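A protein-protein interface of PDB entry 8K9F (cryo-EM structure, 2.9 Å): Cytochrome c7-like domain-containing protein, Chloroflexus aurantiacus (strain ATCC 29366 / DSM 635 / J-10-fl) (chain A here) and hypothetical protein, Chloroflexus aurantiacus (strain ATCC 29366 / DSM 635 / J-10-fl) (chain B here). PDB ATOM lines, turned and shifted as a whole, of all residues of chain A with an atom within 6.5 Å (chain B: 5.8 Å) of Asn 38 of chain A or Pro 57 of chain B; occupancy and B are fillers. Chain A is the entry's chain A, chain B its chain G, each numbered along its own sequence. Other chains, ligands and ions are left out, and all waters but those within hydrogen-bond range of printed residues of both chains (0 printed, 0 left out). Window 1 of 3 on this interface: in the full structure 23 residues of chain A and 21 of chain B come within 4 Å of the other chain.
Asn 38 of chain A touches three residues of chain B.
Printed residues of chain B within 4 Å of Val 45 of chain A: Pro 57.
Of the printed residues of chain A, Phe 58 of chain B touches Asn 44.
The nearest residue of chain B that does not touch Asn 38 of chain A is Phe 58 of chain B (4.9 Å).
The nearest residue of chain A that does not touch Pro 57 of chain B is Tyr 39 of chain A (4.3 Å).
The side-chain amide oxygen of Asn 44 of chain A is in hydrogen-bond range of the side-chain amide nitrogen of Asn 38 of chain A, at 3.4 Å.
The backbone carbonyl oxygen of Tyr 34 of chain A lies within hydrogen-bond range of the side-chain hydroxyl of Ser 37 of chain A (2.9 Å).
O of Asn 38 of chain A sits at hydrogen-bond distance from N of Val 43 of chain A (2.9 Å).
The side-chain hydroxyl of Ser 37 of chain A is in hydrogen-bond range of the backbone NH of Phe 40 of chain A, at 3.0 Å.
Val 33 of chain A touches Gly 54 of chain B (CG1 to CA, 3.8 Å).
Gly 54 of chain B touches Ser 37 of chain A (O to CA, 3.3 Å).
Arg 55 of chain B touches Asn 38 of chain A (CD to OD1, 3.9 Å).
O of Pro 57 of chain B touches O of Val 43 of chain A (3.8 Å).
Asn 44 of chain A touches Pro 57 of chain B.
Phe 58 of chain B touches Asn 44 of chain A (O to CB, 3.5 Å).
Asn 44 of chain A touches Thr 59 of chain B.
Val 45 of chain A touches Pro 57 of chain B (CG2 to CB, 3.7 Å).
Of the 13 printed residues of chain A, 6 touch a printed residue of chain B.
Among the printed residues, no Asp or Glu carboxylate lies within 4 Å of a Lys or Arg side-chain nitrogen of the other chain.
O of Pro 57 of chain B sits at hydrogen-bond distance from ND2 of Asn 38 of chain A (3.0 Å).
The backbone NH (N) of Asn 38 of chain A sits at hydrogen-bond distance from the backbone carbonyl oxygen (O) of Gly 54 of chain B (3.0 Å).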
ATOM      1  N   VAL A  33     -24.305  13.241   2.750  1.00  0.00           N
ATOM      2  CA  VAL A  33     -23.912  14.532   3.302  1.00  0.00           C
ATOM      3  C   VAL A  33     -23.334  15.421   2.210  1.00  0.00           C
ATOM      4  O   VAL A  33     -23.681  16.602   2.113  1.00  0.00           O
ATOM      5  CB  VAL A  33     -22.927  14.335   4.472  1.00  0.00           C
ATOM      6  CG1 VAL A  33     -22.038  15.557   4.678  1.00  0.00           C
ATOM      7  CG2 VAL A  33     -23.685  14.030   5.747  1.00  0.00           C
ATOM      8  N   TYR A  34     -22.484  14.855   1.342  1.00  0.00           N
ATOM      9  CA  TYR A  34     -21.896  15.648   0.267  1.00  0.00           C
ATOM     10  C   TYR A  34     -22.936  16.094  -0.751  1.00  0.00           C
ATOM     11  O   TYR A  34     -22.839  17.206  -1.275  1.00  0.00           O
ATOM     12  CB  TYR A  34     -20.788  14.876  -0.445  1.00  0.00           C
ATOM     13  CG  TYR A  34     -20.056  15.724  -1.464  1.00  0.00           C
ATOM     14  CD1 TYR A  34     -19.140  16.687  -1.062  1.00  0.00           C
ATOM     15  CD2 TYR A  34     -20.291  15.575  -2.823  1.00  0.00           C
ATOM     16  CE1 TYR A  34     -18.474  17.468  -1.982  1.00  0.00           C
ATOM     17  CE2 TYR A  34     -19.634  16.351  -3.749  1.00  0.00           C
ATOM     18  CZ  TYR A  34     -18.726  17.294  -3.326  1.00  0.00           C
ATOM     19  OH  TYR A  34     -18.066  18.069  -4.253  1.00  0.00           O
ATOM     20  N   ARG A  36     -25.944  16.835  -0.018  1.00  0.00           N
ATOM     21  CA  ARG A  36     -26.826  17.818   0.584  1.00  0.00           C
ATOM     22  C   ARG A  36     -26.019  18.925   1.194  1.00  0.00           C
ATOM     23  O   ARG A  36     -26.562  19.820   1.819  1.00  0.00           O
ATOM     24  CB  ARG A  36     -27.694  17.150   1.642  1.00  0.00           C
ATOM     25  CG  ARG A  36     -28.891  16.431   1.065  1.00  0.00           C
ATOM     26  CD  ARG A  36     -29.213  15.171   1.842  1.00  0.00           C
ATOM     27  NE  ARG A  36     -29.975  14.231   1.031  1.00  0.00           N
ATOM     28  CZ  ARG A  36     -29.428  13.422   0.133  1.00  0.00           C
ATOM     29  NH1 ARG A  36     -28.124  13.453  -0.064  1.00  0.00           N
ATOM     30  NH2 ARG A  36     -30.178  12.592  -0.571  1.00  0.00           N
ATOM     31  N   SER A  37     -24.723  18.904   0.970  1.00  0.00           N
ATOM     32  CA  SER A  37     -23.860  19.854   1.650  1.00  0.00           C
ATOM     33  C   SER A  37     -24.093  21.274   1.155  1.00  0.00           C
ATOM     34  O   SER A  37     -24.486  21.513   0.012  1.00  0.00           O
ATOM     35  CB  SER A  37     -22.390  19.487   1.468  1.00  0.00           C
ATOM     36  OG  SER A  37     -21.982  19.637   0.126  1.00  0.00           O
ATOM     37  N   ASN A  38     -23.829  22.228   2.045  1.00  0.00           N
ATOM     38  CA  ASN A  38     -23.858  23.637   1.694  1.00  0.00           C
ATOM     39  C   ASN A  38     -22.716  24.036   0.775  1.00  0.00           C
ATOM     40  O   ASN A  38     -22.774  25.112   0.181  1.00  0.00           O
ATOM     41  CB  ASN A  38     -23.820  24.498   2.956  1.00  0.00           C
ATOM     42  CG  ASN A  38     -25.154  24.562   3.653  1.00  0.00           C
ATOM     43  OD1 ASN A  38     -26.116  23.924   3.234  1.00  0.00           O
ATOM     44  ND2 ASN A  38     -25.226  25.343   4.721  1.00  0.00           N
ATOM     45  N   TYR A  39     -21.670  23.215   0.667  1.00  0.00           N
ATOM     46  CA  TYR A  39     -20.664  23.444  -0.361  1.00  0.00           C
ATOM     47  C   TYR A  39     -21.192  23.079  -1.740  1.00  0.00           C
ATOM     48  O   TYR A  39     -20.970  23.817  -2.706  1.00  0.00           O
ATOM     49  CB  TYR A  39     -19.404  22.639  -0.065  1.00  0.00           C
ATOM     50  CG  TYR A  39     -18.395  22.708  -1.180  1.00  0.00           C
ATOM     51  CD1 TYR A  39     -17.875  23.926  -1.590  1.00  0.00           C
ATOM     52  CD2 TYR A  39     -17.978  21.561  -1.838  1.00  0.00           C
ATOM     53  CE1 TYR A  39     -16.962  23.999  -2.614  1.00  0.00           C
ATOM     54  CE2 TYR A  39     -17.062  21.622  -2.862  1.00  0.00           C
ATOM     55  CZ  TYR A  39     -16.558  22.845  -3.246  1.00  0.00           C
ATOM     56  OH  TYR A  39     -15.642  22.919  -4.267  1.00  0.00           O
ATOM     57  N   PHE A  40     -21.868  21.933  -1.849  1.00  0.00           N
ATOM     58  CA  PHE A  40     -22.305  21.416  -3.143  1.00  0.00           C
ATOM     59  C   PHE A  40     -23.356  22.317  -3.769  1.00  0.00           C
ATOM     60  O   PHE A  40     -23.205  22.760  -4.911  1.00  0.00           O
ATOM     61  CB  PHE A  40     -22.848  20.000  -2.975  1.00  0.00           C
ATOM     62  CG  PHE A  40     -23.037  19.254  -4.258  1.00  0.00           C
ATOM     63  CD1 PHE A  40     -21.981  19.055  -5.126  1.00  0.00           C
ATOM     64  CD2 PHE A  40     -24.278  18.739  -4.590  1.00  0.00           C
ATOM     65  CE1 PHE A  40     -22.162  18.362  -6.307  1.00  0.00           C
ATOM     66  CE2 PHE A  40     -24.463  18.042  -5.771  1.00  0.00           C
ATOM     67  CZ  PHE A  40     -23.403  17.856  -6.628  1.00  0.00           C
ATOM     68  N   ARG A  41     -24.395  22.644  -3.020  1.00  0.00           N
ATOM     69  CA  ARG A  41     -25.468  23.469  -3.540  1.00  0.00           C
ATOM     70  C   ARG A  41     -25.201  24.958  -3.388  1.00  0.00           C
ATOM     71  O   ARG A  41     -26.044  25.758  -3.805  1.00  0.00           O
ATOM     72  CB  ARG A  41     -26.780  23.101  -2.857  1.00  0.00           C
ATOM     73  CG  ARG A  41     -27.003  21.620  -2.682  1.00  0.00           C
ATOM     74  CD  ARG A  41     -27.422  20.979  -3.987  1.00  0.00           C
ATOM     75  NE  ARG A  41     -28.353  21.810  -4.736  1.00  0.00           N
ATOM     76  CZ  ARG A  41     -29.331  21.343  -5.499  1.00  0.00           C
ATOM     77  NH1 ARG A  41     -29.547  20.046  -5.629  1.00  0.00           N
ATOM     78  NH2 ARG A  41     -30.113  22.200  -6.147  1.00  0.00           N
ATOM     79  N   GLN A  42     -24.049  25.328  -2.815  1.00  0.00           N
ATOM     80  CA  GLN A  42     -23.622  26.711  -2.576  1.00  0.00           C
ATOM     81  C   GLN A  42     -24.651  27.478  -1.744  1.00  0.00           C
ATOM     82  O   GLN A  42     -25.138  28.540  -2.122  1.00  0.00           O
ATOM     83  CB  GLN A  42     -23.305  27.432  -3.891  1.00  0.00           C
ATOM     84  CG  GLN A  42     -22.153  26.824  -4.666  1.00  0.00           C
ATOM     85  CD  GLN A  42     -20.807  27.149  -4.058  1.00  0.00           C
ATOM     86  OE1 GLN A  42     -20.217  28.184  -4.354  1.00  0.00           O
ATOM     87  NE2 GLN A  42     -20.309  26.263  -3.209  1.00  0.00           N
ATOM     88  N   VAL A  43     -24.965  26.910  -0.588  1.00  0.00           N
ATOM     89  CA  VAL A  43     -25.996  27.427   0.300  1.00  0.00           C
ATOM     90  C   VAL A  43     -25.314  28.141   1.454  1.00  0.00           C
ATOM     91  O   VAL A  43     -24.339  27.626   2.015  1.00  0.00           O
ATOM     92  CB  VAL A  43     -26.908  26.294   0.795  1.00  0.00           C
ATOM     93  CG1 VAL A  43     -27.930  26.797   1.783  1.00  0.00           C
ATOM     94  CG2 VAL A  43     -27.601  25.677  -0.372  1.00  0.00           C
ATOM     95  N   ASN A  44     -25.816  29.338   1.780  1.00  0.00           N
ATOM     96  CA  ASN A  44     -25.255  30.244   2.785  1.00  0.00           C
ATOM     97  C   ASN A  44     -23.815  30.614   2.457  1.00  0.00           C
ATOM     98  O   ASN A  44     -22.981  30.769   3.349  1.00  0.00           O
ATOM     99  CB  ASN A  44     -25.370  29.670   4.202  1.00  0.00           C
ATOM    100  CG  ASN A  44     -26.794  29.327   4.572  1.00  0.00           C
ATOM    101  OD1 ASN A  44     -27.139  28.162   4.732  1.00  0.00           O
ATOM    102  ND2 ASN A  44     -27.633  30.342   4.698  1.00  0.00           N
ATOM    103  N   VAL A  45     -23.526  30.753   1.168  1.00  0.00           N
ATOM    104  CA  VAL A  45     -22.239  31.215   0.673  1.00  0.00           C
ATOM    105  C   VAL A  45     -22.498  32.510  -0.082  1.00  0.00           C
ATOM    106  O   VAL A  45     -23.265  32.526  -1.053  1.00  0.00           O
ATOM    107  CB  VAL A  45     -21.565  30.166  -0.226  1.00  0.00           C
ATOM    108  CG1 VAL A  45     -20.471  30.793  -1.076  1.00  0.00           C
ATOM    109  CG2 VAL A  45     -21.008  29.035   0.613  1.00  0.00           C
ATOM    110  N   ALA A 158     -31.091  25.278  -0.488  1.00  0.00           N
ATOM    111  CA  ALA A 158     -30.913  24.643  -1.782  1.00  0.00           C
ATOM    112  C   ALA A 158     -32.261  24.472  -2.460  1.00  0.00           C
ATOM    113  O   ALA A 158     -33.229  24.032  -1.835  1.00  0.00           O
ATOM    114  CB  ALA A 158     -30.219  23.302  -1.615  1.00  0.00           C
ATOM    115  N   ALA B  53     -19.901  19.145   8.884  1.00  0.00           N
ATOM    116  CA  ALA B  53     -19.167  19.600   7.713  1.00  0.00           C
ATOM    117  C   ALA B  53     -20.051  19.748   6.485  1.00  0.00           C
ATOM    118  O   ALA B  53     -19.690  20.495   5.573  1.00  0.00           O
ATOM    119  CB  ALA B  53     -18.017  18.639   7.407  1.00  0.00           C
ATOM    120  N   GLY B  54     -21.179  19.059   6.427  1.00  0.00           N
ATOM    121  CA  GLY B  54     -22.142  19.321   5.382  1.00  0.00           C
ATOM    122  C   GLY B  54     -22.970  20.565   5.612  1.00  0.00           C
ATOM    123  O   GLY B  54     -23.715  20.981   4.723  1.00  0.00           O
ATOM    124  N   ARG B  55     -22.886  21.154   6.804  1.00  0.00           N
ATOM    125  CA  ARG B  55     -23.421  22.486   7.047  1.00  0.00           C
ATOM    126  C   ARG B  55     -22.308  23.467   7.386  1.00  0.00           C
ATOM    127  O   ARG B  55     -22.572  24.459   8.078  1.00  0.00           O
ATOM    128  CB  ARG B  55     -24.453  22.464   8.179  1.00  0.00           C
ATOM    129  CG  ARG B  55     -25.698  21.653   7.886  1.00  0.00           C
ATOM    130  CD  ARG B  55     -26.397  22.142   6.641  1.00  0.00           C
ATOM    131  NE  ARG B  55     -27.632  21.412   6.384  1.00  0.00           N
ATOM    132  CZ  ARG B  55     -28.829  21.801   6.800  1.00  0.00           C
ATOM    133  NH1 ARG B  55     -28.987  22.909   7.505  1.00  0.00           N
ATOM    134  NH2 ARG B  55     -29.893  21.063   6.501  1.00  0.00           N
ATOM    135  N   LEU B  56     -21.078  23.201   6.945  1.00  0.00           N
ATOM    136  CA  LEU B  56     -19.920  24.006   7.333  1.00  0.00           C
ATOM    137  C   LEU B  56     -19.982  25.460   6.864  1.00  0.00           C
ATOM    138  O   LEU B  56     -19.545  26.335   7.629  1.00  0.00           O
ATOM    139  CB  LEU B  56     -18.637  23.292   6.867  1.00  0.00           C
ATOM    140  CG  LEU B  56     -17.229  23.727   7.291  1.00  0.00           C
ATOM    141  CD1 LEU B  56     -16.602  24.705   6.291  1.00  0.00           C
ATOM    142  CD2 LEU B  56     -17.213  24.291   8.714  1.00  0.00           C
ATOM    143  N   PRO B  57     -20.487  25.807   5.664  1.00  0.00           N
ATOM    144  CA  PRO B  57     -20.870  27.210   5.463  1.00  0.00           C
ATOM    145  C   PRO B  57     -22.151  27.531   6.210  1.00  0.00           C
ATOM    146  O   PRO B  57     -23.247  27.393   5.660  1.00  0.00           O
ATOM    147  CB  PRO B  57     -21.044  27.319   3.945  1.00  0.00           C
ATOM    148  CG  PRO B  57     -20.211  26.247   3.407  1.00  0.00           C
ATOM    149  CD  PRO B  57     -20.420  25.117   4.363  1.00  0.00           C
ATOM    150  N   PHE B  58     -22.023  27.913   7.481  1.00  0.00           N
ATOM    151  CA  PHE B  58     -23.178  28.281   8.291  1.00  0.00           C
ATOM    152  C   PHE B  58     -23.829  29.554   7.768  1.00  0.00           C
ATOM    153  O   PHE B  58     -23.255  30.278   6.949  1.00  0.00           O
ATOM    154  CB  PHE B  58     -22.777  28.485   9.753  1.00  0.00           C
ATOM    155  CG  PHE B  58     -22.573  27.211  10.513  1.00  0.00           C
ATOM    156  CD1 PHE B  58     -21.342  26.577  10.510  1.00  0.00           C
ATOM    157  CD2 PHE B  58     -23.611  26.649  11.238  1.00  0.00           C
ATOM    158  CE1 PHE B  58     -21.151  25.400  11.207  1.00  0.00           C
ATOM    159  CE2 PHE B  58     -23.426  25.472  11.941  1.00  0.00           C
ATOM    160  CZ  PHE B  58     -22.193  24.847  11.923  1.00  0.00           C
ATOM    161  N   THR B  59     -25.046  29.807   8.250  1.00  0.00           N
ATOM    162  CA  THR B  59     -25.818  30.968   7.835  1.00  0.00           C
ATOM    163  C   THR B  59     -25.086  32.245   8.240  1.00  0.00           C
ATOM    164  O   THR B  59     -24.659  32.364   9.397  1.00  0.00           O
ATOM    165  CB  THR B  59     -27.206  30.943   8.475  1.00  0.00           C
ATOM    166  OG1 THR B  59     -27.742  29.617   8.415  1.00  0.00           O
ATOM    167  CG2 THR B  59     -28.145  31.895   7.754  1.00  0.00           C
